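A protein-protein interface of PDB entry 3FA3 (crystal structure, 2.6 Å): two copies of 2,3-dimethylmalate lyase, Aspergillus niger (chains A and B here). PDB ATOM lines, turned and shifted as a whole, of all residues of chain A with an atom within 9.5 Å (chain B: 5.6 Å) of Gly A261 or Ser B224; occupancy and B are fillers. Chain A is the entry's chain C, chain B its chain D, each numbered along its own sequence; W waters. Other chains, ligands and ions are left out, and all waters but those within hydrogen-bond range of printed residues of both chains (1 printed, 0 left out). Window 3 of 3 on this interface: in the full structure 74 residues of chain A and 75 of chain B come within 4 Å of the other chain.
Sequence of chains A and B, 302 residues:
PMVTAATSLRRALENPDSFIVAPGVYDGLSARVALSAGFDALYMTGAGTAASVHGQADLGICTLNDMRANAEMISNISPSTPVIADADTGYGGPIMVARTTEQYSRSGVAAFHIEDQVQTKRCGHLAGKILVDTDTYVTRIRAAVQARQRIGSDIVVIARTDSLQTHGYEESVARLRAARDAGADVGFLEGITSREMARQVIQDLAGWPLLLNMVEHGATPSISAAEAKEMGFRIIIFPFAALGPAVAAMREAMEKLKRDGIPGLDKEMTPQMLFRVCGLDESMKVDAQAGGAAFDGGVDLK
The backbone NH (N) of Ala B225 is in hydrogen-bond range of the backbone carbonyl oxygen (O) of Gly A261.
The backbone carbonyl oxygen (O) of Pro A263 sits close to the side-chain amino group (NZ) of Lys A256 (3.3 Å). The side-chain sulfur (SD) of Met B214 lies close to the backbone NH (N) of Ile B223. OG of Ser B224 lies close to N of Glu B227 (3.4 Å).
Leu A257 touches Phe B238. Ser B224 touches Gly A261. O of Gly A261 touches CZ of Phe B238, at 3.4 Å. Ile A262 touches Met B214 (CD1 to CG, 3.6 Å). Ile A262 touches Ile B223 (CD1 to O, 3.2 Å). Pro A263 touches Phe B238 (CG to CD2, 3.7 Å).
Of the printed residues of chain B, Leu A257 touches Phe B238 (3.96 Å). Of the printed residues of chain B, Ile A262 touches Met B214 (3.6 Å) and Ile B223 (3.2 Å). Ser B224 touches just one residue of chain A: Gly A261. Of chain A, only Gly A261 (2.8 Å) comes within 4 Å of Ala B225. No residue of chain A comes within 4 Å of Ala B226. The nearest residue of chain B that does not touch Gly A261 is Ile B223 (4.6 Å).
Printed residues of chain B that touch a printed residue of chain A: Met B214, Ile B223, Ser B224, Ala B225 and Phe B238. Printed residues of chain A that touch a printed residue of chain B: Leu A257, Gly A261, Ile A262 and Pro A263. Hydrophobic or aromatic side chains of chain A within 4 Å of the printed part of chain B: Leu A257, Ile A262 and Pro A263. Among the printed residues, 7 pairs touch across the chains. Among the printed residues, no Asp or Glu carboxylate lies within 4 Å of a Lys or Arg side-chain nitrogen of the other chain.
No position is printed for both chains. Of the 7 pairs that touch across the chains among the printed residues, none has its exchanged pair printed and touching as well.
Water W1 lies within hydrogen-bond range of the backbone NH of Ala B226, the backbone carbonyl oxygen of Asp A260 and the backbone NH of Ala B225.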
ATOM      1  N   ALA A 253      -5.016  18.368 -15.800  1.00  0.00           N
ATOM      2  CA  ALA A 253      -5.662  17.068 -15.821  1.00  0.00           C
ATOM      3  C   ALA A 253      -6.188  16.692 -14.439  1.00  0.00           C
ATOM      4  O   ALA A 253      -7.319  16.206 -14.321  1.00  0.00           O
ATOM      5  CB  ALA A 253      -4.710  15.995 -16.410  1.00  0.00           C
ATOM      6  N   MET A 254      -5.378  16.958 -13.408  1.00  0.00           N
ATOM      7  CA  MET A 254      -5.793  16.795 -12.002  1.00  0.00           C
ATOM      8  C   MET A 254      -6.939  17.687 -11.594  1.00  0.00           C
ATOM      9  O   MET A 254      -7.794  17.271 -10.797  1.00  0.00           O
ATOM     10  CB  MET A 254      -4.673  17.054 -11.021  1.00  0.00           C
ATOM     11  CG  MET A 254      -3.648  16.043 -11.033  1.00  0.00           C
ATOM     12  SD  MET A 254      -4.213  14.493 -10.361  1.00  0.00           S
ATOM     13  CE  MET A 254      -2.897  13.427 -11.024  1.00  0.00           C
ATOM     14  N   GLU A 255      -6.949  18.911 -12.106  1.00  0.00           N
ATOM     15  CA  GLU A 255      -8.082  19.775 -11.884  1.00  0.00           C
ATOM     16  C   GLU A 255      -9.349  19.195 -12.526  1.00  0.00           C
ATOM     17  O   GLU A 255     -10.402  19.170 -11.882  1.00  0.00           O
ATOM     18  CB  GLU A 255      -7.772  21.196 -12.342  1.00  0.00           C
ATOM     19  CG  GLU A 255      -7.649  22.144 -11.163  1.00  0.00           C
ATOM     20  CD  GLU A 255      -6.276  22.772 -11.047  1.00  0.00           C
ATOM     21  OE1 GLU A 255      -5.700  23.131 -12.120  1.00  0.00           O
ATOM     22  OE2 GLU A 255      -5.768  22.906  -9.882  1.00  0.00           O
ATOM     23  N   LYS A 256      -9.229  18.687 -13.757  1.00  0.00           N
ATOM     24  CA  LYS A 256     -10.357  18.072 -14.439  1.00  0.00           C
ATOM     25  C   LYS A 256     -10.856  16.870 -13.660  1.00  0.00           C
ATOM     26  O   LYS A 256     -12.029  16.772 -13.358  1.00  0.00           O
ATOM     27  CB  LYS A 256      -9.976  17.686 -15.862  1.00  0.00           C
ATOM     28  CG  LYS A 256     -11.128  17.225 -16.745  1.00  0.00           C
ATOM     29  CD  LYS A 256     -10.580  16.736 -18.091  1.00  0.00           C
ATOM     30  CE  LYS A 256     -11.502  15.651 -18.706  1.00  0.00           C
ATOM     31  NZ  LYS A 256     -11.042  15.060 -19.994  1.00  0.00           N
ATOM     32  N   LEU A 257      -9.958  15.968 -13.320  1.00  0.00           N
ATOM     33  CA  LEU A 257     -10.287  14.815 -12.502  1.00  0.00           C
ATOM     34  C   LEU A 257     -11.084  15.200 -11.263  1.00  0.00           C
ATOM     35  O   LEU A 257     -12.136  14.608 -11.003  1.00  0.00           O
ATOM     36  CB  LEU A 257      -9.023  14.034 -12.085  1.00  0.00           C
ATOM     37  CG  LEU A 257      -9.353  12.681 -11.417  1.00  0.00           C
ATOM     38  CD1 LEU A 257     -10.230  11.767 -12.274  1.00  0.00           C
ATOM     39  CD2 LEU A 257      -8.104  11.982 -11.003  1.00  0.00           C
ATOM     40  N   LYS A 258     -10.587  16.173 -10.497  1.00  0.00           N
ATOM     41  CA  LYS A 258     -11.334  16.648  -9.311  1.00  0.00           C
ATOM     42  C   LYS A 258     -12.799  17.060  -9.581  1.00  0.00           C
ATOM     43  O   LYS A 258     -13.651  16.686  -8.809  1.00  0.00           O
ATOM     44  CB  LYS A 258     -10.564  17.743  -8.545  1.00  0.00           C
ATOM     45  CG  LYS A 258     -10.100  17.341  -7.165  1.00  0.00           C
ATOM     46  CD  LYS A 258     -10.786  18.170  -6.096  1.00  0.00           C
ATOM     47  CE  LYS A 258     -11.262  17.253  -4.955  1.00  0.00           C
ATOM     48  NZ  LYS A 258     -11.826  17.990  -3.761  1.00  0.00           N
ATOM     49  N   ARG A 259     -13.096  17.815 -10.650  1.00  0.00           N
ATOM     50  CA  ARG A 259     -14.466  18.215 -10.922  1.00  0.00           C
ATOM     51  C   ARG A 259     -15.172  17.014 -11.499  1.00  0.00           C
ATOM     52  O   ARG A 259     -16.291  16.722 -11.113  1.00  0.00           O
ATOM     53  CB  ARG A 259     -14.560  19.409 -11.857  1.00  0.00           C
ATOM     54  CG  ARG A 259     -13.854  20.653 -11.284  1.00  0.00           C
ATOM     55  CD  ARG A 259     -13.662  21.860 -12.298  1.00  0.00           C
ATOM     56  NE  ARG A 259     -13.264  21.395 -13.628  1.00  0.00           N
ATOM     57  CZ  ARG A 259     -12.093  21.614 -14.232  1.00  0.00           C
ATOM     58  NH1 ARG A 259     -11.125  22.364 -13.684  1.00  0.00           N
ATOM     59  NH2 ARG A 259     -11.899  21.053 -15.423  1.00  0.00           N
ATOM     60  N   ASP A 260     -14.502  16.268 -12.370  1.00  0.00           N
ATOM     61  CA  ASP A 260     -15.190  15.236 -13.178  1.00  0.00           C
ATOM     62  C   ASP A 260     -15.313  13.829 -12.581  1.00  0.00           C
ATOM     63  O   ASP A 260     -16.271  13.124 -12.868  1.00  0.00           O
ATOM     64  CB  ASP A 260     -14.590  15.175 -14.582  1.00  0.00           C
ATOM     65  CG  ASP A 260     -14.950  16.384 -15.402  1.00  0.00           C
ATOM     66  OD1 ASP A 260     -15.681  17.262 -14.839  1.00  0.00           O
ATOM     67  OD2 ASP A 260     -14.496  16.444 -16.599  1.00  0.00           O
ATOM     68  N   GLY A 261     -14.340  13.415 -11.780  1.00  0.00           N
ATOM     69  CA  GLY A 261     -14.385  12.094 -11.165  1.00  0.00           C
ATOM     70  C   GLY A 261     -14.016  10.927 -12.070  1.00  0.00           C
ATOM     71  O   GLY A 261     -14.109   9.768 -11.670  1.00  0.00           O
ATOM     72  N   ILE A 262     -13.622  11.238 -13.293  1.00  0.00           N
ATOM     73  CA  ILE A 262     -13.093  10.272 -14.224  1.00  0.00           C
ATOM     74  C   ILE A 262     -12.168  11.071 -15.121  1.00  0.00           C
ATOM     75  O   ILE A 262     -12.530  12.154 -15.578  1.00  0.00           O
ATOM     76  CB  ILE A 262     -14.191   9.526 -14.998  1.00  0.00           C
ATOM     77  CG1 ILE A 262     -13.605   8.444 -15.872  1.00  0.00           C
ATOM     78  CG2 ILE A 262     -14.933  10.433 -15.882  1.00  0.00           C
ATOM     79  CD1 ILE A 262     -13.790   7.108 -15.395  1.00  0.00           C
ATOM     80  N   PRO A 263     -10.967  10.555 -15.388  1.00  0.00           N
ATOM     81  CA  PRO A 263      -9.929  11.413 -15.961  1.00  0.00           C
ATOM     82  C   PRO A 263     -10.236  11.889 -17.354  1.00  0.00           C
ATOM     83  O   PRO A 263      -9.835  12.984 -17.741  1.00  0.00           O
ATOM     84  CB  PRO A 263      -8.697  10.502 -15.990  1.00  0.00           C
ATOM     85  CG  PRO A 263      -9.045   9.371 -15.039  1.00  0.00           C
ATOM     86  CD  PRO A 263     -10.500   9.176 -15.235  1.00  0.00           C
ATOM     87  N   GLY A 264     -10.971  11.046 -18.079  1.00  0.00           N
ATOM     88  CA  GLY A 264     -11.290  11.217 -19.493  1.00  0.00           C
ATOM     89  C   GLY A 264     -10.051  11.343 -20.369  1.00  0.00           C
ATOM     90  O   GLY A 264      -9.900  12.358 -21.030  1.00  0.00           O
ATOM     91  N   ARG B 195     -20.401  -3.393 -15.645  1.00  0.00           N
ATOM     92  CA  ARG B 195     -21.175  -2.932 -14.512  1.00  0.00           C
ATOM     93  C   ARG B 195     -21.906  -4.066 -13.786  1.00  0.00           C
ATOM     94  O   ARG B 195     -21.916  -4.072 -12.551  1.00  0.00           O
ATOM     95  CB  ARG B 195     -22.090  -1.796 -14.920  1.00  0.00           C
ATOM     96  CG  ARG B 195     -21.326  -0.509 -15.143  1.00  0.00           C
ATOM     97  CD  ARG B 195     -22.197   0.677 -15.607  1.00  0.00           C
ATOM     98  NE  ARG B 195     -21.532   1.354 -16.732  1.00  0.00           N
ATOM     99  CZ  ARG B 195     -20.828   2.486 -16.665  1.00  0.00           C
ATOM    100  NH1 ARG B 195     -20.665   3.169 -15.529  1.00  0.00           N
ATOM    101  NH2 ARG B 195     -20.304   2.968 -17.768  1.00  0.00           N
ATOM    102  N   MET B 214      -9.770   2.126 -12.082  1.00  0.00           N
ATOM    103  CA  MET B 214     -10.362   2.764 -13.196  1.00  0.00           C
ATOM    104  C   MET B 214      -9.253   3.167 -14.128  1.00  0.00           C
ATOM    105  O   MET B 214      -8.979   4.371 -14.332  1.00  0.00           O
ATOM    106  CB  MET B 214     -11.202   3.929 -12.743  1.00  0.00           C
ATOM    107  CG  MET B 214     -12.121   4.393 -13.800  1.00  0.00           C
ATOM    108  SD  MET B 214     -12.885   3.109 -14.833  1.00  0.00           S
ATOM    109  CE  MET B 214     -14.095   2.506 -13.689  1.00  0.00           C
ATOM    110  N   SER B 222     -15.734   2.654 -18.378  1.00  0.00           N
ATOM    111  CA  SER B 222     -15.722   3.893 -17.550  1.00  0.00           C
ATOM    112  C   SER B 222     -16.689   4.079 -16.398  1.00  0.00           C
ATOM    113  O   SER B 222     -17.833   4.315 -16.586  1.00  0.00           O
ATOM    114  CB  SER B 222     -15.777   5.104 -18.425  1.00  0.00           C
ATOM    115  OG  SER B 222     -14.486   5.175 -18.928  1.00  0.00           O
ATOM    116  N   ILE B 223     -16.186   4.046 -15.186  1.00  0.00           N
ATOM    117  CA  ILE B 223     -17.023   4.396 -14.041  1.00  0.00           C
ATOM    118  C   ILE B 223     -16.413   5.580 -13.354  1.00  0.00           C
ATOM    119  O   ILE B 223     -15.250   5.535 -12.956  1.00  0.00           O
ATOM    120  CB  ILE B 223     -17.255   3.204 -13.066  1.00  0.00           C
ATOM    121  CG1 ILE B 223     -18.063   2.133 -13.784  1.00  0.00           C
ATOM    122  CG2 ILE B 223     -17.947   3.648 -11.852  1.00  0.00           C
ATOM    123  CD1 ILE B 223     -17.577   0.715 -13.564  1.00  0.00           C
ATOM    124  N   SER B 224     -17.207   6.647 -13.279  1.00  0.00           N
ATOM    125  CA  SER B 224     -16.895   7.840 -12.493  1.00  0.00           C
ATOM    126  C   SER B 224     -16.824   7.486 -11.021  1.00  0.00           C
ATOM    127  O   SER B 224     -17.420   6.490 -10.524  1.00  0.00           O
ATOM    128  CB  SER B 224     -17.990   8.874 -12.669  1.00  0.00           C
ATOM    129  OG  SER B 224     -19.209   8.314 -12.226  1.00  0.00           O
ATOM    130  N   ALA B 225     -16.075   8.311 -10.319  1.00  0.00           N
ATOM    131  CA  ALA B 225     -15.937   8.168  -8.912  1.00  0.00           C
ATOM    132  C   ALA B 225     -17.337   8.169  -8.218  1.00  0.00           C
ATOM    133  O   ALA B 225     -17.620   7.295  -7.406  1.00  0.00           O
ATOM    134  CB  ALA B 225     -15.044   9.286  -8.416  1.00  0.00           C
ATOM    135  N   ALA B 226     -18.222   9.101  -8.560  1.00  0.00           N
ATOM    136  CA  ALA B 226     -19.520   9.145  -7.891  1.00  0.00           C
ATOM    137  C   ALA B 226     -20.276   7.815  -8.006  1.00  0.00           C
ATOM    138  O   ALA B 226     -20.793   7.302  -7.010  1.00  0.00           O
ATOM    139  CB  ALA B 226     -20.386  10.325  -8.391  1.00  0.00           C
ATOM    140  N   GLU B 227     -20.305   7.258  -9.219  1.00  0.00           N
ATOM    141  CA  GLU B 227     -21.066   6.050  -9.518  1.00  0.00           C
ATOM    142  C   GLU B 227     -20.459   4.884  -8.763  1.00  0.00           C
ATOM    143  O   GLU B 227     -21.159   4.001  -8.275  1.00  0.00           O
ATOM    144  CB  GLU B 227     -21.048   5.785 -11.017  1.00  0.00           C
ATOM    145  CG  GLU B 227     -21.596   4.439 -11.387  1.00  0.00           C
ATOM    146  CD  GLU B 227     -21.748   4.241 -12.893  1.00  0.00           C
ATOM    147  OE1 GLU B 227     -21.280   5.142 -13.689  1.00  0.00           O
ATOM    148  OE2 GLU B 227     -22.335   3.188 -13.288  1.00  0.00           O
ATOM    149  N   ALA B 228     -19.135   4.883  -8.671  1.00  0.00           N
ATOM    150  CA  ALA B 228     -18.461   3.842  -7.933  1.00  0.00           C
ATOM    151  C   ALA B 228     -18.827   3.912  -6.434  1.00  0.00           C
ATOM    152  O   ALA B 228     -19.163   2.899  -5.821  1.00  0.00           O
ATOM    153  CB  ALA B 228     -16.967   3.937  -8.153  1.00  0.00           C
ATOM    154  N   LYS B 229     -18.768   5.108  -5.848  1.00  0.00           N
ATOM    155  CA  LYS B 229     -19.169   5.279  -4.464  1.00  0.00           C
ATOM    156  C   LYS B 229     -20.532   4.654  -4.421  1.00  0.00           C
ATOM    157  O   LYS B 229     -20.793   3.783  -3.619  1.00  0.00           O
ATOM    158  CB  LYS B 229     -19.217   6.765  -4.067  1.00  0.00           C
ATOM    159  CG  LYS B 229     -19.324   7.014  -2.583  1.00  0.00           C
ATOM    160  CD  LYS B 229     -19.473   8.486  -2.199  1.00  0.00           C
ATOM    161  CE  LYS B 229     -20.059   8.564  -0.767  1.00  0.00           C
ATOM    162  NZ  LYS B 229     -20.075   9.900  -0.090  1.00  0.00           N
ATOM    163  N   ILE B 236     -11.483   4.138  -5.324  1.00  0.00           N
ATOM    164  CA  ILE B 236     -11.324   4.096  -6.785  1.00  0.00           C
ATOM    165  C   ILE B 236      -9.921   4.645  -7.134  1.00  0.00           C
ATOM    166  O   ILE B 236      -9.467   5.653  -6.506  1.00  0.00           O
ATOM    167  CB  ILE B 236     -12.437   4.880  -7.519  1.00  0.00           C
ATOM    168  CG1 ILE B 236     -12.287   4.695  -9.032  1.00  0.00           C
ATOM    169  CG2 ILE B 236     -12.512   6.404  -7.027  1.00  0.00           C
ATOM    170  CD1 ILE B 236     -13.444   5.321  -9.881  1.00  0.00           C
ATOM    171  N   PHE B 238      -6.873   5.726 -10.197  1.00  0.00           N
ATOM    172  CA  PHE B 238      -6.813   6.254 -11.548  1.00  0.00           C
ATOM    173  C   PHE B 238      -5.369   6.165 -12.019  1.00  0.00           C
ATOM    174  O   PHE B 238      -4.707   7.219 -12.204  1.00  0.00           O
ATOM    175  CB  PHE B 238      -7.350   7.678 -11.573  1.00  0.00           C
ATOM    176  CG  PHE B 238      -8.791   7.788 -11.167  1.00  0.00           C
ATOM    177  CD1 PHE B 238      -9.146   8.310  -9.934  1.00  0.00           C
ATOM    178  CD2 PHE B 238      -9.815   7.350 -12.014  1.00  0.00           C
ATOM    179  CE1 PHE B 238     -10.500   8.420  -9.567  1.00  0.00           C
ATOM    180  CE2 PHE B 238     -11.140   7.466 -11.639  1.00  0.00           C
ATOM    181  CZ  PHE B 238     -11.475   8.002 -10.421  1.00  0.00           C
HETATM  182  O   HOH W   1     -17.377  11.474 -10.252  1.00  0.00           O
